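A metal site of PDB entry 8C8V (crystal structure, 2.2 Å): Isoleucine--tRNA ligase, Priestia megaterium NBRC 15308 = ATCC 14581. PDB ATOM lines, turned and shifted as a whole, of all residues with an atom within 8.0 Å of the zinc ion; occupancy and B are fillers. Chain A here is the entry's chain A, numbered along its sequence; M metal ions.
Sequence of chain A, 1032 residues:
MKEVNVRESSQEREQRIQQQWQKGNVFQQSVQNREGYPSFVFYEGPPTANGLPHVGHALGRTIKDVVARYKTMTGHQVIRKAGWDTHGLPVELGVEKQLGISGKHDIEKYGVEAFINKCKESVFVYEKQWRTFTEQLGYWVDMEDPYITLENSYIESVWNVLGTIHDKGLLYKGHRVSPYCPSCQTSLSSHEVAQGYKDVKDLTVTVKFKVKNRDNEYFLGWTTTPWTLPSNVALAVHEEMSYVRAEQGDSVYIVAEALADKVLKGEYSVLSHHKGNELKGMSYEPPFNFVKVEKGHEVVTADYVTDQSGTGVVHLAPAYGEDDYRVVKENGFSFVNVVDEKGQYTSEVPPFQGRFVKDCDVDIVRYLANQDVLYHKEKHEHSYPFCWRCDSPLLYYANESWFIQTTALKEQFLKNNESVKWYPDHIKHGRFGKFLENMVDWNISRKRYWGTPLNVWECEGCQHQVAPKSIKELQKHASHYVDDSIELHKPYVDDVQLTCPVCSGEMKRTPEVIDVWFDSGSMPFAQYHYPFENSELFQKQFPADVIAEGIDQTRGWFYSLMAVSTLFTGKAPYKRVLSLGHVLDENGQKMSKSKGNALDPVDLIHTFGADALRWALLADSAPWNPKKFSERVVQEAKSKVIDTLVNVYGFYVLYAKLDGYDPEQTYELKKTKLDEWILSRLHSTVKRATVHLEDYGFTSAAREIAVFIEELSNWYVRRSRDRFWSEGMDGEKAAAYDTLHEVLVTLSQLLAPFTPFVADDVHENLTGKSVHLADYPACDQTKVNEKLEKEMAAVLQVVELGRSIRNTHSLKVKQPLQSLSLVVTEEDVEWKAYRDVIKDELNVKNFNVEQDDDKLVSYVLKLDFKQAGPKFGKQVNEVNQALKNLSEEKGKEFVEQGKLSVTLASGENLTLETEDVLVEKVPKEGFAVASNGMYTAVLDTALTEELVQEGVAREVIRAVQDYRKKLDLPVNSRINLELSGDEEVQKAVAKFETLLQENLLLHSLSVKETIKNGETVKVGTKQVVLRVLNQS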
ATOM      1  N   LEU A  89      -1.612  21.136 -23.489  1.00  0.00           N
ATOM      2  CA  LEU A  89      -0.273  21.079 -22.891  1.00  0.00           C
ATOM      3  C   LEU A  89      -0.041  22.120 -21.811  1.00  0.00           C
ATOM      4  O   LEU A  89       0.566  21.772 -20.783  1.00  0.00           O
ATOM      5  CB  LEU A  89       0.790  21.226 -23.999  1.00  0.00           C
ATOM      6  CG  LEU A  89       0.986  20.074 -24.977  1.00  0.00           C
ATOM      7  CD1 LEU A  89       1.713  20.554 -26.229  1.00  0.00           C
ATOM      8  CD2 LEU A  89       1.768  18.945 -24.304  1.00  0.00           C
ATOM      9  N   LEU A  93       1.159  19.744 -18.509  1.00  0.00           N
ATOM     10  CA  LEU A  93       2.533  19.693 -18.006  1.00  0.00           C
ATOM     11  C   LEU A  93       2.602  20.105 -16.544  1.00  0.00           C
ATOM     12  O   LEU A  93       3.275  19.443 -15.736  1.00  0.00           O
ATOM     13  CB  LEU A  93       3.437  20.567 -18.860  1.00  0.00           C
ATOM     14  CG  LEU A  93       3.594  20.123 -20.322  1.00  0.00           C
ATOM     15  CD1 LEU A  93       4.621  20.990 -21.022  1.00  0.00           C
ATOM     16  CD2 LEU A  93       3.976  18.658 -20.415  1.00  0.00           C
ATOM     17  N   TYR A 180       8.224  18.667 -34.068  1.00  0.00           N
ATOM     18  CA  TYR A 180       7.860  17.634 -33.125  1.00  0.00           C
ATOM     19  C   TYR A 180       8.616  17.837 -31.824  1.00  0.00           C
ATOM     20  O   TYR A 180       9.826  18.093 -31.839  1.00  0.00           O
ATOM     21  CB  TYR A 180       8.154  16.244 -33.704  1.00  0.00           C
ATOM     22  CG  TYR A 180       7.760  15.083 -32.822  1.00  0.00           C
ATOM     23  CD1 TYR A 180       6.459  14.623 -32.789  1.00  0.00           C
ATOM     24  CD2 TYR A 180       8.707  14.434 -32.041  1.00  0.00           C
ATOM     25  CE1 TYR A 180       6.094  13.542 -31.983  1.00  0.00           C
ATOM     26  CE2 TYR A 180       8.366  13.372 -31.237  1.00  0.00           C
ATOM     27  CZ  TYR A 180       7.062  12.930 -31.216  1.00  0.00           C
ATOM     28  OH  TYR A 180       6.720  11.859 -30.411  1.00  0.00           O
ATOM     29  N   CYS A 181       7.908  17.734 -30.695  1.00  0.00           N
ATOM     30  CA  CYS A 181       8.557  17.852 -29.392  1.00  0.00           C
ATOM     31  C   CYS A 181       8.856  16.461 -28.847  1.00  0.00           C
ATOM     32  O   CYS A 181       7.920  15.712 -28.543  1.00  0.00           O
ATOM     33  CB  CYS A 181       7.683  18.618 -28.407  1.00  0.00           C
ATOM     34  SG  CYS A 181       8.456  18.741 -26.775  1.00  0.00           S
ATOM     35  N   PRO A 182      10.127  16.076 -28.715  1.00  0.00           N
ATOM     36  CA  PRO A 182      10.448  14.743 -28.186  1.00  0.00           C
ATOM     37  C   PRO A 182      10.080  14.553 -26.719  1.00  0.00           C
ATOM     38  O   PRO A 182       9.925  13.404 -26.289  1.00  0.00           O
ATOM     39  CB  PRO A 182      11.962  14.623 -28.413  1.00  0.00           C
ATOM     40  CG  PRO A 182      12.443  16.042 -28.400  1.00  0.00           C
ATOM     41  CD  PRO A 182      11.335  16.859 -29.037  1.00  0.00           C
ATOM     42  N   SER A 183       9.951  15.626 -25.940  1.00  0.00           N
ATOM     43  CA  SER A 183       9.557  15.489 -24.543  1.00  0.00           C
ATOM     44  C   SER A 183       8.037  15.326 -24.407  1.00  0.00           C
ATOM     45  O   SER A 183       7.554  14.327 -23.887  1.00  0.00           O
ATOM     46  CB  SER A 183      10.037  16.685 -23.735  1.00  0.00           C
ATOM     47  OG  SER A 183       9.602  16.574 -22.388  1.00  0.00           O
ATOM     48  N   CYS A 184       7.286  16.326 -24.882  1.00  0.00           N
ATOM     49  CA  CYS A 184       5.829  16.211 -24.889  1.00  0.00           C
ATOM     50  C   CYS A 184       5.354  15.067 -25.772  1.00  0.00           C
ATOM     51  O   CYS A 184       4.229  14.585 -25.585  1.00  0.00           O
ATOM     52  CB  CYS A 184       5.191  17.529 -25.360  1.00  0.00           C
ATOM     53  SG  CYS A 184       5.511  18.966 -24.304  1.00  0.00           S
ATOM     54  N   GLN A 185       6.193  14.620 -26.717  1.00  0.00           N
ATOM     55  CA  GLN A 185       5.887  13.504 -27.624  1.00  0.00           C
ATOM     56  C   GLN A 185       4.666  13.805 -28.487  1.00  0.00           C
ATOM     57  O   GLN A 185       3.741  13.001 -28.613  1.00  0.00           O
ATOM     58  CB  GLN A 185       5.705  12.198 -26.846  1.00  0.00           C
ATOM     59  CG  GLN A 185       6.964  11.716 -26.125  1.00  0.00           C
ATOM     60  CD  GLN A 185       6.762  10.393 -25.414  1.00  0.00           C
ATOM     61  OE1 GLN A 185       6.382   9.399 -26.023  1.00  0.00           O
ATOM     62  NE2 GLN A 185       7.005  10.383 -24.100  1.00  0.00           N
ATOM     63  N   THR A 186       4.678  14.976 -29.119  1.00  0.00           N
ATOM     64  CA  THR A 186       3.587  15.358 -30.006  1.00  0.00           C
ATOM     65  C   THR A 186       4.092  16.351 -31.043  1.00  0.00           C
ATOM     66  O   THR A 186       5.024  17.119 -30.795  1.00  0.00           O
ATOM     67  CB  THR A 186       2.413  15.962 -29.233  1.00  0.00           C
ATOM     68  OG1 THR A 186       1.294  16.124 -30.107  1.00  0.00           O
ATOM     69  CG2 THR A 186       2.794  17.318 -28.638  1.00  0.00           C
ATOM     70  N   LEU A 188       3.525  19.785 -33.283  1.00  0.00           N
ATOM     71  CA  LEU A 188       3.089  21.117 -32.909  1.00  0.00           C
ATOM     72  C   LEU A 188       2.733  21.909 -34.151  1.00  0.00           C
ATOM     73  O   LEU A 188       3.197  21.614 -35.260  1.00  0.00           O
ATOM     74  CB  LEU A 188       4.167  21.875 -32.109  1.00  0.00           C
ATOM     75  CG  LEU A 188       4.583  21.285 -30.760  1.00  0.00           C
ATOM     76  CD1 LEU A 188       5.735  22.081 -30.196  1.00  0.00           C
ATOM     77  CD2 LEU A 188       3.403  21.277 -29.801  1.00  0.00           C
ATOM     78  N   PHE A 386      12.349  25.534 -30.252  1.00  0.00           N
ATOM     79  CA  PHE A 386      12.180  24.845 -28.980  1.00  0.00           C
ATOM     80  C   PHE A 386      10.706  24.787 -28.621  1.00  0.00           C
ATOM     81  O   PHE A 386       9.914  25.644 -29.052  1.00  0.00           O
ATOM     82  CB  PHE A 386      12.964  25.548 -27.863  1.00  0.00           C
ATOM     83  CG  PHE A 386      14.455  25.412 -27.989  1.00  0.00           C
ATOM     84  CD1 PHE A 386      15.159  26.166 -28.917  1.00  0.00           C
ATOM     85  CD2 PHE A 386      15.153  24.538 -27.171  1.00  0.00           C
ATOM     86  CE1 PHE A 386      16.520  26.037 -29.040  1.00  0.00           C
ATOM     87  CE2 PHE A 386      16.528  24.409 -27.289  1.00  0.00           C
ATOM     88  CZ  PHE A 386      17.209  25.154 -28.216  1.00  0.00           C
ATOM     89  N   CYS A 387      10.328  23.785 -27.840  1.00  0.00           N
ATOM     90  CA  CYS A 387       8.937  23.660 -27.424  1.00  0.00           C
ATOM     91  C   CYS A 387       8.523  24.848 -26.571  1.00  0.00           C
ATOM     92  O   CYS A 387       9.143  25.135 -25.547  1.00  0.00           O
ATOM     93  CB  CYS A 387       8.720  22.355 -26.652  1.00  0.00           C
ATOM     94  SG  CYS A 387       7.048  22.230 -25.953  1.00  0.00           S
ATOM     95  N   TRP A 388       7.454  25.529 -26.990  1.00  0.00           N
ATOM     96  CA  TRP A 388       6.994  26.731 -26.294  1.00  0.00           C
ATOM     97  C   TRP A 388       6.489  26.440 -24.886  1.00  0.00           C
ATOM     98  O   TRP A 388       6.273  27.386 -24.121  1.00  0.00           O
ATOM     99  CB  TRP A 388       5.901  27.414 -27.111  1.00  0.00           C
ATOM    100  CG  TRP A 388       4.593  26.666 -27.122  1.00  0.00           C
ATOM    101  CD1 TRP A 388       4.365  25.414 -27.621  1.00  0.00           C
ATOM    102  CD2 TRP A 388       3.339  27.139 -26.620  1.00  0.00           C
ATOM    103  NE1 TRP A 388       3.042  25.074 -27.446  1.00  0.00           N
ATOM    104  CE2 TRP A 388       2.380  26.114 -26.840  1.00  0.00           C
ATOM    105  CE3 TRP A 388       2.917  28.319 -26.005  1.00  0.00           C
ATOM    106  CZ2 TRP A 388       1.048  26.243 -26.455  1.00  0.00           C
ATOM    107  CZ3 TRP A 388       1.590  28.447 -25.633  1.00  0.00           C
ATOM    108  CH2 TRP A 388       0.671  27.408 -25.859  1.00  0.00           C
ATOM    109  N   ARG A 389       6.278  25.174 -24.529  1.00  0.00           N
ATOM    110  CA  ARG A 389       5.845  24.843 -23.172  1.00  0.00           C
ATOM    111  C   ARG A 389       6.971  24.255 -22.303  1.00  0.00           C
ATOM    112  O   ARG A 389       7.199  24.745 -21.197  1.00  0.00           O
ATOM    113  CB  ARG A 389       4.657  23.873 -23.205  1.00  0.00           C
ATOM    114  CG  ARG A 389       3.420  24.435 -23.922  1.00  0.00           C
ATOM    115  CD  ARG A 389       3.064  25.847 -23.438  1.00  0.00           C
ATOM    116  NE  ARG A 389       2.926  25.954 -21.996  1.00  0.00           N
ATOM    117  CZ  ARG A 389       2.576  27.063 -21.351  1.00  0.00           C
ATOM    118  NH1 ARG A 389       2.286  28.178 -22.004  1.00  0.00           N
ATOM    119  NH2 ARG A 389       2.528  27.060 -20.026  1.00  0.00           N
ATOM    120  N   CYS A 390       7.663  23.221 -22.768  1.00  0.00           N
ATOM    121  CA  CYS A 390       8.637  22.516 -21.939  1.00  0.00           C
ATOM    122  C   CYS A 390      10.093  22.851 -22.262  1.00  0.00           C
ATOM    123  O   CYS A 390      10.993  22.264 -21.653  1.00  0.00           O
ATOM    124  CB  CYS A 390       8.434  20.999 -22.046  1.00  0.00           C
ATOM    125  SG  CYS A 390       9.048  20.280 -23.579  1.00  0.00           S
ATOM    126  N   ASP A 391      10.338  23.771 -23.195  1.00  0.00           N
ATOM    127  CA  ASP A 391      11.673  24.269 -23.557  1.00  0.00           C
ATOM    128  C   ASP A 391      12.579  23.198 -24.150  1.00  0.00           C
ATOM    129  O   ASP A 391      13.773  23.442 -24.344  1.00  0.00           O
ATOM    130  CB  ASP A 391      12.375  24.926 -22.365  1.00  0.00           C
ATOM    131  CG  ASP A 391      12.205  26.431 -22.351  1.00  0.00           C
ATOM    132  OD1 ASP A 391      12.416  27.063 -23.416  1.00  0.00           O
ATOM    133  OD2 ASP A 391      11.873  26.986 -21.283  1.00  0.00           O
ATOM    134  N   SER A 392      12.064  22.008 -24.446  1.00  0.00           N
ATOM    135  CA  SER A 392      12.878  21.012 -25.115  1.00  0.00           C
ATOM    136  C   SER A 392      13.140  21.443 -26.558  1.00  0.00           C
ATOM    137  O   SER A 392      12.268  22.025 -27.201  1.00  0.00           O
ATOM    138  CB  SER A 392      12.197  19.648 -25.097  1.00  0.00           C
ATOM    139  OG  SER A 392      12.728  18.798 -26.093  1.00  0.00           O
ATOM    140  N   PRO A 393      14.337  21.171 -27.089  1.00  0.00           N
ATOM    141  CA  PRO A 393      14.562  21.404 -28.517  1.00  0.00           C
ATOM    142  C   PRO A 393      13.624  20.542 -29.349  1.00  0.00           C
ATOM    143  O   PRO A 393      13.320  19.403 -28.985  1.00  0.00           O
ATOM    144  CB  PRO A 393      16.026  21.007 -28.715  1.00  0.00           C
ATOM    145  CG  PRO A 393      16.312  20.053 -27.591  1.00  0.00           C
ATOM    146  CD  PRO A 393      15.508  20.574 -26.437  1.00  0.00           C
ATOM    147  N   LEU A 394      13.152  21.106 -30.449  1.00  0.00           N
ATOM    148  CA  LEU A 394      12.244  20.380 -31.319  1.00  0.00           C
ATOM    149  C   LEU A 394      13.029  19.563 -32.346  1.00  0.00           C
ATOM    150  O   LEU A 394      14.218  19.774 -32.568  1.00  0.00           O
ATOM    151  CB  LEU A 394      11.295  21.318 -32.051  1.00  0.00           C
ATOM    152  CG  LEU A 394      10.317  22.142 -31.213  1.00  0.00           C
ATOM    153  CD1 LEU A 394       9.329  22.868 -32.126  1.00  0.00           C
ATOM    154  CD2 LEU A 394       9.595  21.255 -30.220  1.00  0.00           C
ATOM    155  N   ARG A 448      -2.143  13.407 -26.928  1.00  0.00           N
ATOM    156  CA  ARG A 448      -2.216  13.709 -25.512  1.00  0.00           C
ATOM    157  C   ARG A 448      -3.582  13.286 -24.967  1.00  0.00           C
ATOM    158  O   ARG A 448      -4.330  12.583 -25.658  1.00  0.00           O
ATOM    159  CB  ARG A 448      -1.971  15.202 -25.255  1.00  0.00           C
ATOM    160  CG  ARG A 448      -0.621  15.702 -25.756  1.00  0.00           C
ATOM    161  CD  ARG A 448       0.532  15.135 -24.956  1.00  0.00           C
ATOM    162  NE  ARG A 448       0.464  15.547 -23.554  1.00  0.00           N
ATOM    163  CZ  ARG A 448       1.455  15.401 -22.678  1.00  0.00           C
ATOM    164  NH1 ARG A 448       2.604  14.852 -23.026  1.00  0.00           N
ATOM    165  NH2 ARG A 448       1.275  15.829 -21.435  1.00  0.00           N
HETATM  166 ZN    ZN M   1       7.373  20.055 -25.209  1.00  0.00          ZN
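The backbone carbonyl oxygen (O) of Ser 392 is in hydrogen-bond range of the backbone NH (N) of Cys 387. SG of Cys 387 sits close to N of Arg 389. The backbone carbonyl oxygen (O) of Thr 186 is in hydrogen-bond range of the backbone NH (N) of Cys 181, at 3.0 Å. The side-chain sulfur (SG) of Cys 181 lies close to the backbone NH (N) of Ser 183, 3.6 Å away. O of Cys 184 is in hydrogen-bond range of NH1 of Arg 448, at 3.0 Å. SG of Cys 390 sits close to N of Ser 392, at 3.6 Å.
The zinc ion is bound by SG of Cys 181, SG of Cys 387, SG of Cys 184 and SG of Cys 390. The zinc ion has four donor atoms within binding distance.
Within 4 Å of the zinc ion: Cys 181, Cys 184, Cys 387 and Cys 390. The nearest printed residue that does not touch the zinc ion is Ser 183 (4.5 Å).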
